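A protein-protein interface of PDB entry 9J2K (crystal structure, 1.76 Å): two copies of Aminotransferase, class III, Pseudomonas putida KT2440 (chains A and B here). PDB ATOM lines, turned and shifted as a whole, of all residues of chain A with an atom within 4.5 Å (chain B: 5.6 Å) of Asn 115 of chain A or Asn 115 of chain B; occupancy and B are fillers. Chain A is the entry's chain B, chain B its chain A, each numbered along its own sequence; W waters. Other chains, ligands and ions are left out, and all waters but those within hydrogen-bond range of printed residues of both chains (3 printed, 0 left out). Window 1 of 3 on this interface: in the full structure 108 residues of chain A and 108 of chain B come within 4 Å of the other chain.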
ATOM      1  N   THR A 114      16.550 -29.069  22.576  1.00  0.00           N
ATOM      2  CA  THR A 114      15.188 -29.157  22.066  1.00  0.00           C
ATOM      3  C   THR A 114      14.946 -27.947  21.176  1.00  0.00           C
ATOM      4  O   THR A 114      15.829 -27.112  20.981  1.00  0.00           O
ATOM      5  CB  THR A 114      14.153 -29.195  23.199  1.00  0.00           C
ATOM      6  OG1 THR A 114      14.162 -27.938  23.884  1.00  0.00           O
ATOM      7  CG2 THR A 114      14.465 -30.301  24.184  1.00  0.00           C
ATOM      8  N   ASN A 115      13.736 -27.847  20.636  1.00  0.00           N
ATOM      9  CA  ASN A 115      13.370 -26.678  19.845  1.00  0.00           C
ATOM     10  C   ASN A 115      12.862 -25.539  20.716  1.00  0.00           C
ATOM     11  O   ASN A 115      13.164 -24.370  20.451  1.00  0.00           O
ATOM     12  CB  ASN A 115      12.273 -27.032  18.827  1.00  0.00           C
ATOM     13  CG  ASN A 115      12.611 -28.244  17.991  1.00  0.00           C
ATOM     14  OD1 ASN A 115      13.499 -28.194  17.139  1.00  0.00           O
ATOM     15  ND2 ASN A 115      11.886 -29.337  18.209  1.00  0.00           N
ATOM     16  N   SER A 116      12.086 -25.850  21.752  1.00  0.00           N
ATOM     17  CA  SER A 116      11.355 -24.831  22.490  1.00  0.00           C
ATOM     18  C   SER A 116      11.599 -24.972  23.984  1.00  0.00           C
ATOM     19  O   SER A 116      11.996 -26.035  24.475  1.00  0.00           O
ATOM     20  CB  SER A 116       9.849 -24.930  22.233  1.00  0.00           C
ATOM     21  OG  SER A 116       9.359 -26.147  22.785  1.00  0.00           O
ATOM     22  N   GLU A 119       9.250 -27.757  25.283  1.00  0.00           N
ATOM     23  CA  GLU A 119       9.854 -29.081  25.146  1.00  0.00           C
ATOM     24  C   GLU A 119      10.962 -29.306  26.168  1.00  0.00           C
ATOM     25  O   GLU A 119      11.115 -30.416  26.700  1.00  0.00           O
ATOM     26  CB  GLU A 119      10.433 -29.268  23.748  1.00  0.00           C
ATOM     27  CG  GLU A 119       9.441 -29.377  22.628  1.00  0.00           C
ATOM     28  CD  GLU A 119      10.154 -29.170  21.318  1.00  0.00           C
ATOM     29  OE1 GLU A 119      11.296 -28.668  21.371  1.00  0.00           O
ATOM     30  OE2 GLU A 119       9.601 -29.514  20.255  1.00  0.00           O
ATOM     31  N   PRO A 294      14.532 -21.647  16.285  1.00  0.00           N
ATOM     32  CA  PRO A 294      13.970 -22.299  17.477  1.00  0.00           C
ATOM     33  C   PRO A 294      15.005 -23.203  18.133  1.00  0.00           C
ATOM     34  O   PRO A 294      15.472 -24.155  17.506  1.00  0.00           O
ATOM     35  CB  PRO A 294      12.777 -23.103  16.924  1.00  0.00           C
ATOM     36  CG  PRO A 294      12.541 -22.560  15.529  1.00  0.00           C
ATOM     37  CD  PRO A 294      13.894 -22.122  15.043  1.00  0.00           C
ATOM     38  N   LEU A 295      15.404 -22.904  19.369  1.00  0.00           N
ATOM     39  CA  LEU A 295      16.366 -23.736  20.079  1.00  0.00           C
ATOM     40  C   LEU A 295      16.152 -23.558  21.573  1.00  0.00           C
ATOM     41  O   LEU A 295      15.878 -22.447  22.033  1.00  0.00           O
ATOM     42  CB  LEU A 295      17.820 -23.363  19.731  1.00  0.00           C
ATOM     43  CG  LEU A 295      18.875 -24.318  20.291  1.00  0.00           C
ATOM     44  CD1 LEU A 295      18.756 -25.683  19.602  1.00  0.00           C
ATOM     45  CD2 LEU A 295      20.265 -23.738  20.080  1.00  0.00           C
ATOM     46  N   ALA A 296      16.285 -24.651  22.317  1.00  0.00           N
ATOM     47  CA  ALA A 296      16.368 -24.583  23.768  1.00  0.00           C
ATOM     48  C   ALA A 296      17.373 -25.626  24.230  1.00  0.00           C
ATOM     49  O   ALA A 296      17.755 -26.528  23.471  1.00  0.00           O
ATOM     50  CB  ALA A 296      15.001 -24.791  24.441  1.00  0.00           C
ATOM     51  N   LEU A 322      13.795 -35.276  19.903  1.00  0.00           N
ATOM     52  CA  LEU A 322      13.024 -34.603  18.873  1.00  0.00           C
ATOM     53  C   LEU A 322      13.779 -34.669  17.556  1.00  0.00           C
ATOM     54  O   LEU A 322      15.014 -34.690  17.528  1.00  0.00           O
ATOM     55  CB  LEU A 322      12.770 -33.148  19.242  1.00  0.00           C
ATOM     56  CG  LEU A 322      12.120 -33.011  20.619  1.00  0.00           C
ATOM     57  CD1 LEU A 322      12.422 -31.661  21.204  1.00  0.00           C
ATOM     58  CD2 LEU A 322      10.629 -33.253  20.508  1.00  0.00           C
ATOM     59  N   CYS A 324      14.451 -32.504  15.414  1.00  0.00           N
ATOM     60  CA  CYS A 324      15.395 -31.423  15.204  1.00  0.00           C
ATOM     61  C   CYS A 324      16.273 -31.159  16.421  1.00  0.00           C
ATOM     62  O   CYS A 324      16.940 -30.123  16.468  1.00  0.00           O
ATOM     63  CB  CYS A 324      14.647 -30.151  14.780  1.00  0.00           C
ATOM     64  SG  CYS A 324      14.044 -30.252  13.044  1.00  0.00           S
ATOM     65  N   PHE B 113       0.499 -23.339  14.191  1.00  0.00           N
ATOM     66  CA  PHE B 113       1.891 -23.730  13.981  1.00  0.00           C
ATOM     67  C   PHE B 113       2.609 -24.021  15.290  1.00  0.00           C
ATOM     68  O   PHE B 113       2.401 -23.333  16.295  1.00  0.00           O
ATOM     69  CB  PHE B 113       2.663 -22.641  13.225  1.00  0.00           C
ATOM     70  CG  PHE B 113       2.252 -22.510  11.776  1.00  0.00           C
ATOM     71  CD1 PHE B 113       2.414 -23.574  10.900  1.00  0.00           C
ATOM     72  CD2 PHE B 113       1.701 -21.327  11.304  1.00  0.00           C
ATOM     73  CE1 PHE B 113       2.010 -23.480   9.568  1.00  0.00           C
ATOM     74  CE2 PHE B 113       1.311 -21.214   9.965  1.00  0.00           C
ATOM     75  CZ  PHE B 113       1.471 -22.290   9.097  1.00  0.00           C
ATOM     76  N   THR B 114       3.487 -25.027  15.261  1.00  0.00           N
ATOM     77  CA  THR B 114       4.403 -25.301  16.366  1.00  0.00           C
ATOM     78  C   THR B 114       5.800 -25.517  15.794  1.00  0.00           C
ATOM     79  O   THR B 114       6.017 -25.421  14.586  1.00  0.00           O
ATOM     80  CB  THR B 114       3.983 -26.534  17.182  1.00  0.00           C
ATOM     81  OG1 THR B 114       4.097 -27.708  16.371  1.00  0.00           O
ATOM     82  CG2 THR B 114       2.526 -26.406  17.711  1.00  0.00           C
ATOM     83  N   ASN B 115       6.760 -25.826  16.673  1.00  0.00           N
ATOM     84  CA  ASN B 115       8.098 -26.162  16.192  1.00  0.00           C
ATOM     85  C   ASN B 115       8.217 -27.635  15.820  1.00  0.00           C
ATOM     86  O   ASN B 115       8.887 -27.976  14.834  1.00  0.00           O
ATOM     87  CB  ASN B 115       9.154 -25.844  17.253  1.00  0.00           C
ATOM     88  CG  ASN B 115       9.063 -24.432  17.760  1.00  0.00           C
ATOM     89  OD1 ASN B 115       9.333 -23.478  17.026  1.00  0.00           O
ATOM     90  ND2 ASN B 115       8.700 -24.283  19.032  1.00  0.00           N
ATOM     91  N   SER B 116       7.606 -28.521  16.603  1.00  0.00           N
ATOM     92  CA  SER B 116       7.814 -29.956  16.456  1.00  0.00           C
ATOM     93  C   SER B 116       6.489 -30.699  16.354  1.00  0.00           C
ATOM     94  O   SER B 116       5.437 -30.198  16.762  1.00  0.00           O
ATOM     95  CB  SER B 116       8.589 -30.538  17.638  1.00  0.00           C
ATOM     96  OG  SER B 116       7.848 -30.381  18.851  1.00  0.00           O
ATOM     97  N   GLY B 117       6.575 -31.927  15.837  1.00  0.00           N
ATOM     98  CA  GLY B 117       5.415 -32.811  15.845  1.00  0.00           C
ATOM     99  C   GLY B 117       4.945 -33.129  17.253  1.00  0.00           C
ATOM    100  O   GLY B 117       3.742 -33.251  17.504  1.00  0.00           O
ATOM    101  N   GLU B 119       5.135 -31.112  19.937  1.00  0.00           N
ATOM    102  CA  GLU B 119       4.330 -29.967  20.354  1.00  0.00           C
ATOM    103  C   GLU B 119       2.987 -29.950  19.640  1.00  0.00           C
ATOM    104  O   GLU B 119       1.965 -29.544  20.216  1.00  0.00           O
ATOM    105  CB  GLU B 119       5.051 -28.661  20.051  1.00  0.00           C
ATOM    106  CG  GLU B 119       6.286 -28.365  20.865  1.00  0.00           C
ATOM    107  CD  GLU B 119       7.078 -27.263  20.191  1.00  0.00           C
ATOM    108  OE1 GLU B 119       6.821 -27.000  18.997  1.00  0.00           O
ATOM    109  OE2 GLU B 119       7.926 -26.645  20.849  1.00  0.00           O
ATOM    110  N   SER B 285       4.503 -32.316   9.726  1.00  0.00           N
ATOM    111  CA  SER B 285       5.847 -31.849  10.067  1.00  0.00           C
ATOM    112  C   SER B 285       6.849 -32.546   9.153  1.00  0.00           C
ATOM    113  O   SER B 285       6.474 -32.988   8.064  1.00  0.00           O
ATOM    114  CB  SER B 285       6.168 -32.119  11.547  1.00  0.00           C
ATOM    115  OG  SER B 285       7.347 -31.440  11.950  1.00  0.00           O
ATOM    116  N1  LLP B 286       4.467 -38.140  14.913  1.00  0.00           N
ATOM    117  C2  LLP B 286       5.092 -38.969  14.019  1.00  0.00           C
ATOM    118  C2' LLP B 286       4.267 -39.922  13.208  1.00  0.00           C
ATOM    119  C3  LLP B 286       6.477 -38.916  13.855  1.00  0.00           C
ATOM    120  O3  LLP B 286       7.080 -39.757  12.986  1.00  0.00           O
ATOM    121  C4  LLP B 286       7.256 -38.018  14.588  1.00  0.00           C
ATOM    122  C4' LLP B 286       8.548 -37.561  13.972  1.00  0.00           C
ATOM    123  C5  LLP B 286       6.602 -37.191  15.512  1.00  0.00           C
ATOM    124  C6  LLP B 286       5.228 -37.258  15.665  1.00  0.00           C
ATOM    125  C5' LLP B 286       7.370 -36.231  16.380  1.00  0.00           C
ATOM    126  OP4 LLP B 286       7.877 -35.139  15.664  1.00  0.00           O
ATOM    127  P   LLP B 286       9.055 -34.323  16.407  1.00  0.00           P
ATOM    128  OP1 LLP B 286      10.252 -35.247  16.513  1.00  0.00           O
ATOM    129  OP2 LLP B 286       8.587 -33.954  17.794  1.00  0.00           O
ATOM    130  OP3 LLP B 286       9.341 -33.081  15.604  1.00  0.00           O
ATOM    131  N   LLP B 286       8.115 -32.633   9.585  1.00  0.00           N
ATOM    132  CA  LLP B 286       9.170 -33.369   8.886  1.00  0.00           C
ATOM    133  CB  LLP B 286       8.958 -34.879   9.067  1.00  0.00           C
ATOM    134  CG  LLP B 286       9.335 -35.361  10.487  1.00  0.00           C
ATOM    135  CD  LLP B 286       9.366 -36.906  10.596  1.00  0.00           C
ATOM    136  CE  LLP B 286      10.029 -37.354  11.917  1.00  0.00           C
ATOM    137  NZ  LLP B 286       9.062 -38.112  12.763  1.00  0.00           N
ATOM    138  C   LLP B 286       9.295 -32.978   7.409  1.00  0.00           C
ATOM    139  O   LLP B 286       9.947 -31.979   7.109  1.00  0.00           O
ATOM    140  N   PRO B 294      12.812 -26.214  11.955  1.00  0.00           N
ATOM    141  CA  PRO B 294      11.822 -26.893  12.810  1.00  0.00           C
ATOM    142  C   PRO B 294      10.442 -26.281  12.599  1.00  0.00           C
ATOM    143  O   PRO B 294      10.235 -25.093  12.846  1.00  0.00           O
ATOM    144  CB  PRO B 294      12.343 -26.646  14.235  1.00  0.00           C
ATOM    145  CG  PRO B 294      13.788 -26.197  14.066  1.00  0.00           C
ATOM    146  CD  PRO B 294      13.795 -25.454  12.744  1.00  0.00           C
ATOM    147  N   LEU B 295       9.498 -27.092  12.131  1.00  0.00           N
ATOM    148  CA  LEU B 295       8.137 -26.601  11.964  1.00  0.00           C
ATOM    149  C   LEU B 295       7.166 -27.769  11.984  1.00  0.00           C
ATOM    150  O   LEU B 295       7.457 -28.842  11.454  1.00  0.00           O
ATOM    151  CB  LEU B 295       7.979 -25.820  10.655  1.00  0.00           C
ATOM    152  CG  LEU B 295       6.638 -25.089  10.475  1.00  0.00           C
ATOM    153  CD1 LEU B 295       6.502 -23.931  11.464  1.00  0.00           C
ATOM    154  CD2 LEU B 295       6.491 -24.592   9.031  1.00  0.00           C
ATOM    155  N   ALA B 296       6.007 -27.544  12.586  1.00  0.00           N
ATOM    156  CA  ALA B 296       4.908 -28.488  12.485  1.00  0.00           C
ATOM    157  C   ALA B 296       3.626 -27.680  12.392  1.00  0.00           C
ATOM    158  O   ALA B 296       3.604 -26.482  12.695  1.00  0.00           O
ATOM    159  CB  ALA B 296       4.890 -29.453  13.679  1.00  0.00           C
ATOM    160  N   LEU B 322       3.626 -21.004  21.381  1.00  0.00           N
ATOM    161  CA  LEU B 322       5.066 -21.144  21.534  1.00  0.00           C
ATOM    162  C   LEU B 322       5.743 -19.876  21.038  1.00  0.00           C
ATOM    163  O   LEU B 322       5.255 -19.223  20.113  1.00  0.00           O
ATOM    164  CB  LEU B 322       5.609 -22.347  20.755  1.00  0.00           C
ATOM    165  CG  LEU B 322       5.195 -23.797  21.080  1.00  0.00           C
ATOM    166  CD1 LEU B 322       5.375 -24.118  22.566  1.00  0.00           C
ATOM    167  CD2 LEU B 322       3.790 -24.127  20.613  1.00  0.00           C
ATOM    168  N   CYS B 324       8.169 -19.407  19.126  1.00  0.00           N
ATOM    169  CA  CYS B 324       8.439 -19.403  17.700  1.00  0.00           C
ATOM    170  C   CYS B 324       7.268 -19.911  16.870  1.00  0.00           C
ATOM    171  O   CYS B 324       7.460 -20.198  15.695  1.00  0.00           O
ATOM    172  CB  CYS B 324       9.704 -20.212  17.394  1.00  0.00           C
ATOM    173  SG  CYS B 324      11.219 -19.385  17.993  1.00  0.00           S
ATOM    174  N   THR B 325       6.063 -19.999  17.436  1.00  0.00           N
ATOM    175  CA  THR B 325       4.885 -20.309  16.627  1.00  0.00           C
ATOM    176  C   THR B 325       4.805 -19.375  15.430  1.00  0.00           C
ATOM    177  O   THR B 325       4.834 -18.152  15.582  1.00  0.00           O
ATOM    178  CB  THR B 325       3.615 -20.184  17.473  1.00  0.00           C
ATOM    179  OG1 THR B 325       3.474 -21.364  18.257  1.00  0.00           O
ATOM    180  CG2 THR B 325       2.359 -20.011  16.579  1.00  0.00           C
HETATM  181  O   HOH W   1      12.133 -21.890  20.377  1.00  0.00           O
HETATM  182  O   HOH W   2      11.641 -31.528  16.045  1.00  0.00           O
HETATM  183  O   HOH W   3      10.651 -29.854  13.963  1.00  0.00           O
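Water W1 bridges O of Asn 115 of chain A and SG of Cys 324 of chain B. Water W3 bridges O of Asn 115 of chain B (2.7 Å) and SG of Cys 324 of chain A (3.5 Å). Water W2 lies within hydrogen-bond range of OP3 of LLP 286 of chain B (2.8 Å), the backbone NH of Cys 324 of chain A (3.0 Å) and the side-chain amide nitrogen of Asn 115 of chain A (3.1 Å).
The backbone carbonyl oxygen (O) of Asn 115 of chain A lies within hydrogen-bond range of the backbone NH (N) of Leu 295 of chain A (2.9 Å). OE1 of Glu 119 of chain B is in hydrogen-bond range of N of Ser 116 of chain B. The backbone carbonyl oxygen (O) of Ser 116 of chain A lies within hydrogen-bond range of the side-chain hydroxyl (OG1) of Thr 114 of chain A. The backbone NH (N) of Gly 117 of chain B lies within hydrogen-bond range of OP3 of LLP 286 of chain B (3.0 Å). The backbone NH of Asn 115 of chain A is in hydrogen-bond range of the side-chain carboxylate of Glu 119 of chain A. The backbone NH (N) of Ser 116 of chain A sits at hydrogen-bond distance from the side-chain carboxylate (OE1) of Glu 119 of chain A (3.0 Å).
CB of Asn 115 of chain B touches CB of Asn 115 of chain A, at 3.7 Å. Asn 115 of chain A touches Ser 116 of chain B (ND2 to CB, 3.6 Å). Pro 294 of chain B touches Asn 115 of chain A (CB to OD1, 3.5 Å). Ser 116 of chain A touches Asn 115 of chain B (CB to ND2, 3.5 Å). OD1 of Asn 115 of chain B touches CB of Pro 294 of chain A, 3.5 Å away. Leu 322 of chain A touches LLP 286 of chain B.
Asn 115 of chain B touches its own counterpart, Asn 115 of chain A. Asn 115 of chain A touches Ser 116 of chain B, and with the chains exchanged Ser 116 of chain A touches Asn 115 of chain B. Asn 115 of chain A touches Pro 294 of chain B, and with the chains exchanged Pro 294 of chain A touches Asn 115 of chain B. Ser 116 of chain A touches Glu 119 of chain B, and with the chains exchanged Glu 119 of chain A touches Ser 116 of chain B. Positions printed for both chains: 114, 115, 116, 119, 294, 295, 296, 322 and 324.
The side-chain carboxylate of Glu 119 of chain B is in hydrogen-bond range of the side-chain hydroxyl of Ser 116 of chain A, 2.5 Å away. The side-chain carboxylate of Glu 119 of chain A lies close to the side-chain carboxylate of Glu 119 of chain B, at 3.4 Å. OG of Ser 116 of chain B sits at hydrogen-bond distance from OE2 of Glu 119 of chain A, 2.4 Å away.
Asn 115 of chain A touches just these residues of chain B: Asn 115, Ser 116 and Pro 294. Of chain A, only Asn 115, Ser 116 and Pro 294 come within 4 Å of Asn 115 of chain B. Of the printed residues of chain B, Leu 322 of chain A touches LLP 286 (3.5 Å). Of the printed residues of chain A, Glu 119 of chain B touches Ser 116 (2.5 Å) and Glu 119 (3.4 Å). Printed residues of chain A within 4 Å of Pro 294 of chain B: Asn 115. Thr 114 of chain B touches none of the printed residues of chain A. Gly 117 of chain B touches none of the printed residues of chain A. The nearest residue of chain B that does not touch Asn 115 of chain A is Glu 119 of chain B (4.8 Å). The nearest printed residue of chain A that does not touch Asn 115 of chain B is Glu 119 of chain A (4.8 Å). The nearest printed residue of chain A that does not touch Pro 294 of chain B is Cys 324 of chain A (4.03 Å).
Of the 14 printed residues of chain B, 5 touch a printed residue of chain A. Hydrophobic or aromatic side chains of chain B within 4 Å of the printed part of chain A: Pro 294. Of the 9 printed residues of chain A, 5 touch a printed residue of chain B. Among the printed residues, 9 pairs touch across the chains. Among the printed residues, no Asp or Glu carboxylate lies within 4 Å of a Lys or Arg side-chain nitrogen of the other chain.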
